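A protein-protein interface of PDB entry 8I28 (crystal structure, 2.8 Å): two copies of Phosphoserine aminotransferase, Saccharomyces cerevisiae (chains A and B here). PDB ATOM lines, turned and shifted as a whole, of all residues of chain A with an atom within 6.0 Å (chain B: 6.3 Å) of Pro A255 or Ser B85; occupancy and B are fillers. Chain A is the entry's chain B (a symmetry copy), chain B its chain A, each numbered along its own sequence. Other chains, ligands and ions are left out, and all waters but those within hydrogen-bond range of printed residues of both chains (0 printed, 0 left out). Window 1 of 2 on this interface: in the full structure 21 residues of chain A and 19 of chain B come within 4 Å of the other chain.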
ATOM      1  N   THR A  89     -28.460   6.635  36.623  1.00  0.00           N
ATOM      2  CA  THR A  89     -28.914   7.050  35.296  1.00  0.00           C
ATOM      3  C   THR A  89     -30.023   6.136  34.779  1.00  0.00           C
ATOM      4  O   THR A  89     -30.990   6.616  34.168  1.00  0.00           O
ATOM      5  CB  THR A  89     -27.744   7.099  34.306  1.00  0.00           C
ATOM      6  OG1 THR A  89     -27.016   5.872  34.335  1.00  0.00           O
ATOM      7  CG2 THR A  89     -26.796   8.204  34.671  1.00  0.00           C
ATOM      8  N   ASN A  90     -29.919   4.828  35.038  1.00  0.00           N
ATOM      9  CA  ASN A  90     -30.944   3.901  34.554  1.00  0.00           C
ATOM     10  C   ASN A  90     -32.282   4.105  35.270  1.00  0.00           C
ATOM     11  O   ASN A  90     -33.346   4.022  34.640  1.00  0.00           O
ATOM     12  CB  ASN A  90     -30.476   2.444  34.704  1.00  0.00           C
ATOM     13  CG  ASN A  90     -29.668   1.944  33.494  1.00  0.00           C
ATOM     14  OD1 ASN A  90     -30.223   1.697  32.422  1.00  0.00           O
ATOM     15  ND2 ASN A  90     -28.359   1.765  33.682  1.00  0.00           N
ATOM     16  N   ILE A 253     -27.980  10.235  30.069  1.00  0.00           N
ATOM     17  CA  ILE A 253     -28.183   8.960  29.398  1.00  0.00           C
ATOM     18  C   ILE A 253     -27.092   7.997  29.832  1.00  0.00           C
ATOM     19  O   ILE A 253     -25.902   8.340  29.844  1.00  0.00           O
ATOM     20  CB  ILE A 253     -28.200   9.132  27.869  1.00  0.00           C
ATOM     21  CG1 ILE A 253     -29.036  10.363  27.498  1.00  0.00           C
ATOM     22  CG2 ILE A 253     -28.675   7.847  27.190  1.00  0.00           C
ATOM     23  CD1 ILE A 253     -30.540  10.146  27.521  1.00  0.00           C
ATOM     24  N   THR A 254     -27.496   6.809  30.206  1.00  0.00           N
ATOM     25  CA  THR A 254     -26.529   5.821  30.630  1.00  0.00           C
ATOM     26  C   THR A 254     -25.813   5.266  29.397  1.00  0.00           C
ATOM     27  O   THR A 254     -26.473   4.970  28.387  1.00  0.00           O
ATOM     28  CB  THR A 254     -27.251   4.720  31.439  1.00  0.00           C
ATOM     29  OG1 THR A 254     -26.764   3.431  31.063  1.00  0.00           O
ATOM     30  CG2 THR A 254     -28.810   4.778  31.257  1.00  0.00           C
ATOM     31  N   PRO A 255     -24.475   5.171  29.405  1.00  0.00           N
ATOM     32  CA  PRO A 255     -23.772   4.468  28.319  1.00  0.00           C
ATOM     33  C   PRO A 255     -24.411   3.111  28.058  1.00  0.00           C
ATOM     34  O   PRO A 255     -24.859   2.431  28.989  1.00  0.00           O
ATOM     35  CB  PRO A 255     -22.346   4.319  28.858  1.00  0.00           C
ATOM     36  CG  PRO A 255     -22.182   5.487  29.727  1.00  0.00           C
ATOM     37  CD  PRO A 255     -23.527   5.721  30.386  1.00  0.00           C
ATOM     38  N   ILE A 256     -24.466   2.714  26.781  1.00  0.00           N
ATOM     39  CA  ILE A 256     -25.185   1.477  26.461  1.00  0.00           C
ATOM     40  C   ILE A 256     -24.506   0.277  27.094  1.00  0.00           C
ATOM     41  O   ILE A 256     -25.171  -0.712  27.429  1.00  0.00           O
ATOM     42  CB  ILE A 256     -25.341   1.278  24.944  1.00  0.00           C
ATOM     43  CG1 ILE A 256     -24.549   2.344  24.192  1.00  0.00           C
ATOM     44  CG2 ILE A 256     -26.838   1.248  24.565  1.00  0.00           C
ATOM     45  CD1 ILE A 256     -23.409   1.792  23.392  1.00  0.00           C
ATOM     46  N   ALA A 257     -23.182   0.338  27.274  1.00  0.00           N
ATOM     47  CA  ALA A 257     -22.488  -0.712  28.008  1.00  0.00           C
ATOM     48  C   ALA A 257     -23.152  -1.003  29.358  1.00  0.00           C
ATOM     49  O   ALA A 257     -23.065  -2.130  29.861  1.00  0.00           O
ATOM     50  CB  ALA A 257     -21.018  -0.322  28.175  1.00  0.00           C
ATOM     51  N   PHE A 258     -23.872  -0.022  29.928  1.00  0.00           N
ATOM     52  CA  PHE A 258     -24.514  -0.160  31.232  1.00  0.00           C
ATOM     53  C   PHE A 258     -26.010   0.135  31.199  1.00  0.00           C
ATOM     54  O   PHE A 258     -26.623   0.326  32.256  1.00  0.00           O
ATOM     55  CB  PHE A 258     -23.825   0.739  32.252  1.00  0.00           C
ATOM     56  CG  PHE A 258     -22.386   0.438  32.405  1.00  0.00           C
ATOM     57  CD1 PHE A 258     -21.974  -0.684  33.097  1.00  0.00           C
ATOM     58  CD2 PHE A 258     -21.438   1.235  31.808  1.00  0.00           C
ATOM     59  CE1 PHE A 258     -20.624  -0.985  33.226  1.00  0.00           C
ATOM     60  CE2 PHE A 258     -20.095   0.942  31.927  1.00  0.00           C
ATOM     61  CZ  PHE A 258     -19.684  -0.168  32.639  1.00  0.00           C
ATOM     62  N   ASP A 259     -26.617   0.164  30.020  1.00  0.00           N
ATOM     63  CA  ASP A 259     -28.073   0.270  29.909  1.00  0.00           C
ATOM     64  C   ASP A 259     -28.742  -1.040  30.323  1.00  0.00           C
ATOM     65  O   ASP A 259     -28.919  -1.938  29.501  1.00  0.00           O
ATOM     66  CB  ASP A 259     -28.476   0.606  28.486  1.00  0.00           C
ATOM     67  CG  ASP A 259     -29.870   1.125  28.401  1.00  0.00           C
ATOM     68  OD1 ASP A 259     -30.347   1.742  29.379  1.00  0.00           O
ATOM     69  OD2 ASP A 259     -30.540   0.798  27.413  1.00  0.00           O
ATOM     70  N   THR B  81     -18.299  -0.962  22.851  1.00  0.00           N
ATOM     71  CA  THR B  81     -18.960   0.322  23.032  1.00  0.00           C
ATOM     72  C   THR B  81     -18.306   1.165  24.115  1.00  0.00           C
ATOM     73  O   THR B  81     -18.385   2.392  24.062  1.00  0.00           O
ATOM     74  CB  THR B  81     -20.414   0.085  23.403  1.00  0.00           C
ATOM     75  OG1 THR B  81     -20.512  -0.080  24.830  1.00  0.00           O
ATOM     76  CG2 THR B  81     -20.931  -1.183  22.720  1.00  0.00           C
ATOM     77  N   THR B  82     -17.705   0.529  25.117  1.00  0.00           N
ATOM     78  CA  THR B  82     -17.101   1.254  26.232  1.00  0.00           C
ATOM     79  C   THR B  82     -16.192   2.371  25.740  1.00  0.00           C
ATOM     80  O   THR B  82     -16.142   3.450  26.335  1.00  0.00           O
ATOM     81  CB  THR B  82     -16.313   0.273  27.110  1.00  0.00           C
ATOM     82  OG1 THR B  82     -17.228  -0.584  27.801  1.00  0.00           O
ATOM     83  CG2 THR B  82     -15.412   1.009  28.115  1.00  0.00           C
ATOM     84  N   GLY B  83     -15.479   2.133  24.639  1.00  0.00           N
ATOM     85  CA  GLY B  83     -14.562   3.144  24.138  1.00  0.00           C
ATOM     86  C   GLY B  83     -15.286   4.336  23.538  1.00  0.00           C
ATOM     87  O   GLY B  83     -14.904   5.488  23.773  1.00  0.00           O
ATOM     88  N   PHE B  84     -16.327   4.074  22.733  1.00  0.00           N
ATOM     89  CA  PHE B  84     -17.180   5.150  22.236  1.00  0.00           C
ATOM     90  C   PHE B  84     -17.568   6.070  23.372  1.00  0.00           C
ATOM     91  O   PHE B  84     -17.277   7.269  23.355  1.00  0.00           O
ATOM     92  CB  PHE B  84     -18.479   4.629  21.611  1.00  0.00           C
ATOM     93  CG  PHE B  84     -18.308   3.615  20.537  1.00  0.00           C
ATOM     94  CD1 PHE B  84     -17.085   3.392  19.929  1.00  0.00           C
ATOM     95  CD2 PHE B  84     -19.405   2.871  20.133  1.00  0.00           C
ATOM     96  CE1 PHE B  84     -16.965   2.433  18.940  1.00  0.00           C
ATOM     97  CE2 PHE B  84     -19.293   1.922  19.143  1.00  0.00           C
ATOM     98  CZ  PHE B  84     -18.078   1.701  18.544  1.00  0.00           C
ATOM     99  N   SER B  85     -18.243   5.510  24.368  1.00  0.00           N
ATOM    100  CA  SER B  85     -18.843   6.329  25.398  1.00  0.00           C
ATOM    101  C   SER B  85     -17.780   7.161  26.098  1.00  0.00           C
ATOM    102  O   SER B  85     -17.843   8.396  26.111  1.00  0.00           O
ATOM    103  CB  SER B  85     -19.587   5.429  26.376  1.00  0.00           C
ATOM    104  OG  SER B  85     -20.609   4.720  25.707  1.00  0.00           O
ATOM    105  N   SER B  86     -16.756   6.501  26.630  1.00  0.00           N
ATOM    106  CA  SER B  86     -15.868   7.214  27.532  1.00  0.00           C
ATOM    107  C   SER B  86     -15.009   8.224  26.788  1.00  0.00           C
ATOM    108  O   SER B  86     -14.703   9.276  27.346  1.00  0.00           O
ATOM    109  CB  SER B  86     -15.010   6.236  28.365  1.00  0.00           C
ATOM    110  OG  SER B  86     -14.325   5.250  27.609  1.00  0.00           O
ATOM    111  N   VAL B  87     -14.668   7.968  25.520  1.00  0.00           N
ATOM    112  CA  VAL B  87     -13.808   8.914  24.796  1.00  0.00           C
ATOM    113  C   VAL B  87     -14.540  10.221  24.504  1.00  0.00           C
ATOM    114  O   VAL B  87     -13.926  11.301  24.553  1.00  0.00           O
ATOM    115  CB  VAL B  87     -13.247   8.303  23.492  1.00  0.00           C
ATOM    116  CG1 VAL B  87     -14.020   8.792  22.270  1.00  0.00           C
ATOM    117  CG2 VAL B  87     -11.756   8.621  23.345  1.00  0.00           C
ATOM    118  N   ALA B  88     -15.853  10.158  24.222  1.00  0.00           N
ATOM    119  CA  ALA B  88     -16.583  11.354  23.824  1.00  0.00           C
ATOM    120  C   ALA B  88     -16.799  12.297  25.007  1.00  0.00           C
ATOM    121  O   ALA B  88     -16.500  13.500  24.922  1.00  0.00           O
ATOM    122  CB  ALA B  88     -17.908  10.953  23.190  1.00  0.00           C
ATOM    123  N   THR B  89     -17.317  11.778  26.129  1.00  0.00           N
ATOM    124  CA  THR B  89     -17.561  12.660  27.270  1.00  0.00           C
ATOM    125  C   THR B  89     -16.258  13.107  27.914  1.00  0.00           C
ATOM    126  O   THR B  89     -16.160  14.247  28.382  1.00  0.00           O
ATOM    127  CB  THR B  89     -18.437  11.973  28.311  1.00  0.00           C
ATOM    128  OG1 THR B  89     -17.821  10.747  28.715  1.00  0.00           O
ATOM    129  CG2 THR B  89     -19.781  11.654  27.718  1.00  0.00           C
ATOM    130  N   ASN B  90     -15.254  12.229  27.952  1.00  0.00           N
ATOM    131  CA  ASN B  90     -13.951  12.637  28.461  1.00  0.00           C
ATOM    132  C   ASN B  90     -13.383  13.775  27.640  1.00  0.00           C
ATOM    133  O   ASN B  90     -12.965  14.797  28.187  1.00  0.00           O
ATOM    134  CB  ASN B  90     -12.974  11.463  28.454  1.00  0.00           C
ATOM    135  CG  ASN B  90     -12.969  10.704  29.748  1.00  0.00           C
ATOM    136  OD1 ASN B  90     -12.285  11.072  30.691  1.00  0.00           O
ATOM    137  ND2 ASN B  90     -13.773   9.663  29.815  1.00  0.00           N
ATOM    138  N   GLU B 120     -23.444   6.882  19.221  1.00  0.00           N
ATOM    139  CA  GLU B 120     -23.465   6.804  20.677  1.00  0.00           C
ATOM    140  C   GLU B 120     -23.174   8.160  21.305  1.00  0.00           C
ATOM    141  O   GLU B 120     -23.743   8.505  22.343  1.00  0.00           O
ATOM    142  CB  GLU B 120     -22.465   5.749  21.168  1.00  0.00           C
ATOM    143  CG  GLU B 120     -22.048   5.876  22.648  1.00  0.00           C
ATOM    144  CD  GLU B 120     -23.114   5.370  23.622  1.00  0.00           C
ATOM    145  OE1 GLU B 120     -24.304   5.263  23.221  1.00  0.00           O
ATOM    146  OE2 GLU B 120     -22.756   5.071  24.788  1.00  0.00           O
ATOM    147  N   ARG B 123     -26.529   9.910  21.075  1.00  0.00           N
ATOM    148  CA  ARG B 123     -27.405   9.368  22.101  1.00  0.00           C
ATOM    149  C   ARG B 123     -27.066   9.960  23.458  1.00  0.00           C
ATOM    150  O   ARG B 123     -27.963  10.309  24.236  1.00  0.00           O
ATOM    151  CB  ARG B 123     -27.273   7.843  22.100  1.00  0.00           C
ATOM    152  CG  ARG B 123     -28.076   7.099  23.117  1.00  0.00           C
ATOM    153  CD  ARG B 123     -27.585   5.651  23.215  1.00  0.00           C
ATOM    154  NE  ARG B 123     -28.127   4.941  24.370  1.00  0.00           N
ATOM    155  CZ  ARG B 123     -27.468   4.718  25.496  1.00  0.00           C
ATOM    156  NH1 ARG B 123     -26.206   5.079  25.642  1.00  0.00           N
ATOM    157  NH2 ARG B 123     -28.091   4.118  26.506  1.00  0.00           N
ATOM    158  N   LEU B 124     -25.773  10.135  23.725  1.00  0.00           N
ATOM    159  CA  LEU B 124     -25.282  10.571  25.018  1.00  0.00           C
ATOM    160  C   LEU B 124     -25.440  12.066  25.236  1.00  0.00           C
ATOM    161  O   LEU B 124     -25.257  12.532  26.358  1.00  0.00           O
ATOM    162  CB  LEU B 124     -23.792  10.204  25.164  1.00  0.00           C
ATOM    163  CG  LEU B 124     -23.478   8.729  25.460  1.00  0.00           C
ATOM    164  CD1 LEU B 124     -22.034   8.459  25.898  1.00  0.00           C
ATOM    165  CD2 LEU B 124     -24.452   8.129  26.461  1.00  0.00           C
ATOM    166  N   VAL B 126     -23.297  14.260  23.787  1.00  0.00           N
ATOM    167  CA  VAL B 126     -22.072  14.991  23.487  1.00  0.00           C
ATOM    168  C   VAL B 126     -22.293  15.821  22.223  1.00  0.00           C
ATOM    169  O   VAL B 126     -22.869  15.318  21.247  1.00  0.00           O
ATOM    170  CB  VAL B 126     -20.908  14.030  23.345  1.00  0.00           C
ATOM    171  CG1 VAL B 126     -19.621  14.794  23.490  1.00  0.00           C
ATOM    172  CG2 VAL B 126     -21.036  12.963  24.442  1.00  0.00           C
ATOM    173  N   THR B 254     -18.706  11.840  32.336  1.00  0.00           N
ATOM    174  CA  THR B 254     -18.348  10.433  32.330  1.00  0.00           C
ATOM    175  C   THR B 254     -18.347   9.847  33.749  1.00  0.00           C
ATOM    176  O   THR B 254     -17.800  10.464  34.670  1.00  0.00           O
ATOM    177  CB  THR B 254     -16.989  10.272  31.594  1.00  0.00           C
ATOM    178  OG1 THR B 254     -16.379   9.001  31.885  1.00  0.00           O
ATOM    179  CG2 THR B 254     -16.028  11.515  31.700  1.00  0.00           C
ATOM    180  N   PRO B 255     -18.989   8.689  33.968  1.00  0.00           N
ATOM    181  CA  PRO B 255     -18.843   7.971  35.251  1.00  0.00           C
ATOM    182  C   PRO B 255     -17.379   7.809  35.653  1.00  0.00           C
ATOM    183  O   PRO B 255     -16.532   7.488  34.816  1.00  0.00           O
ATOM    184  CB  PRO B 255     -19.490   6.609  34.956  1.00  0.00           C
ATOM    185  CG  PRO B 255     -20.494   6.908  33.896  1.00  0.00           C
ATOM    186  CD  PRO B 255     -19.855   7.957  33.024  1.00  0.00           C
ATOM    187  N   TYR B 260     -10.901   9.348  32.521  1.00  0.00           N
ATOM    188  CA  TYR B 260      -9.511   9.038  32.197  1.00  0.00           C
ATOM    189  C   TYR B 260      -8.492   9.510  33.234  1.00  0.00           C
ATOM    190  O   TYR B 260      -7.576   8.730  33.535  1.00  0.00           O
ATOM    191  CB  TYR B 260      -9.154   9.579  30.800  1.00  0.00           C
ATOM    192  CG  TYR B 260      -9.886   8.873  29.667  1.00  0.00           C
ATOM    193  CD1 TYR B 260     -10.393   7.583  29.831  1.00  0.00           C
ATOM    194  CD2 TYR B 260     -10.103   9.507  28.443  1.00  0.00           C
ATOM    195  CE1 TYR B 260     -11.078   6.934  28.804  1.00  0.00           C
ATOM    196  CE2 TYR B 260     -10.801   8.865  27.400  1.00  0.00           C
ATOM    197  CZ  TYR B 260     -11.282   7.581  27.596  1.00  0.00           C
ATOM    198  OH  TYR B 260     -11.960   6.937  26.598  1.00  0.00           O
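O of Thr A254 sits at hydrogen-bond distance from NH2 of Arg B123 (2.6 Å).
The backbone NH (N) of Ile A256 sits close to the guanidinium group (NH1) of Arg B123, 3.1 Å away.
O of Thr B82 lies within hydrogen-bond range of OG of Ser B86, 2.9 Å away.
OE1 of Glu B120 lies within salt-bridge range of NH1 of Arg B123.
The side-chain hydroxyl (OG1) of Thr A254 sits at hydrogen-bond distance from the side-chain amide nitrogen (ND2) of Asn A90, 3.5 Å away.
OD1 of Asn A90 sits close to OD1 of Asp A259 (3.0 Å).
OG1 of Thr A254 sits at hydrogen-bond distance from O of Phe A258 (3.3 Å).
N of Asp A259 sits at hydrogen-bond distance from OG1 of Thr A254 (3.4 Å).
4 positions are printed for both chains.
Of the 12 pairs that touch across the chains among the printed residues, none has its exchanged pair printed and touching as well.
Of chain A, only Pro A255 (3.6 Å) comes within 4 Å of Ser B85.
Of the printed residues of chain A, Glu B120 touches Pro A255 (3.7 Å) and Ile A256 (3.1 Å).
Of the printed residues of chain A, Leu B124 touches Ile A253 (3.7 Å).
Of the printed residues of chain B, Ile A253 touches Arg B123 (3.4 Å) and Leu B124 (3.7 Å).
The nearest residue of chain B that does not touch Pro A255 is Leu B124 (4.2 Å).
Along chain A the printed residues that touch a printed residue of chain B span positions 253 to 259.
Among the printed residues, no Asp or Glu carboxylate lies within 4 Å of a Lys or Arg side-chain nitrogen of the other chain.
Among the printed residues, merely in contact across the chains: Ile A253 with Arg B123 (3.4 Å), Ile A253 with Leu B124 (3.7 Å), Pro A255 with Ser B85 (3.6 Å), Pro A255 with Glu B120 (3.7 Å), Pro A255 with Arg B123 (3.6 Å), Ile A256 with Thr B81 (3.4 Å), Ile A256 with Glu B120 (3.1 Å), Ala A257 with Thr B81 (3.4 Å), Ala A257 with Thr B82 (3.8 Å) and Asp A259 with Arg B123 (3.96 Å).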
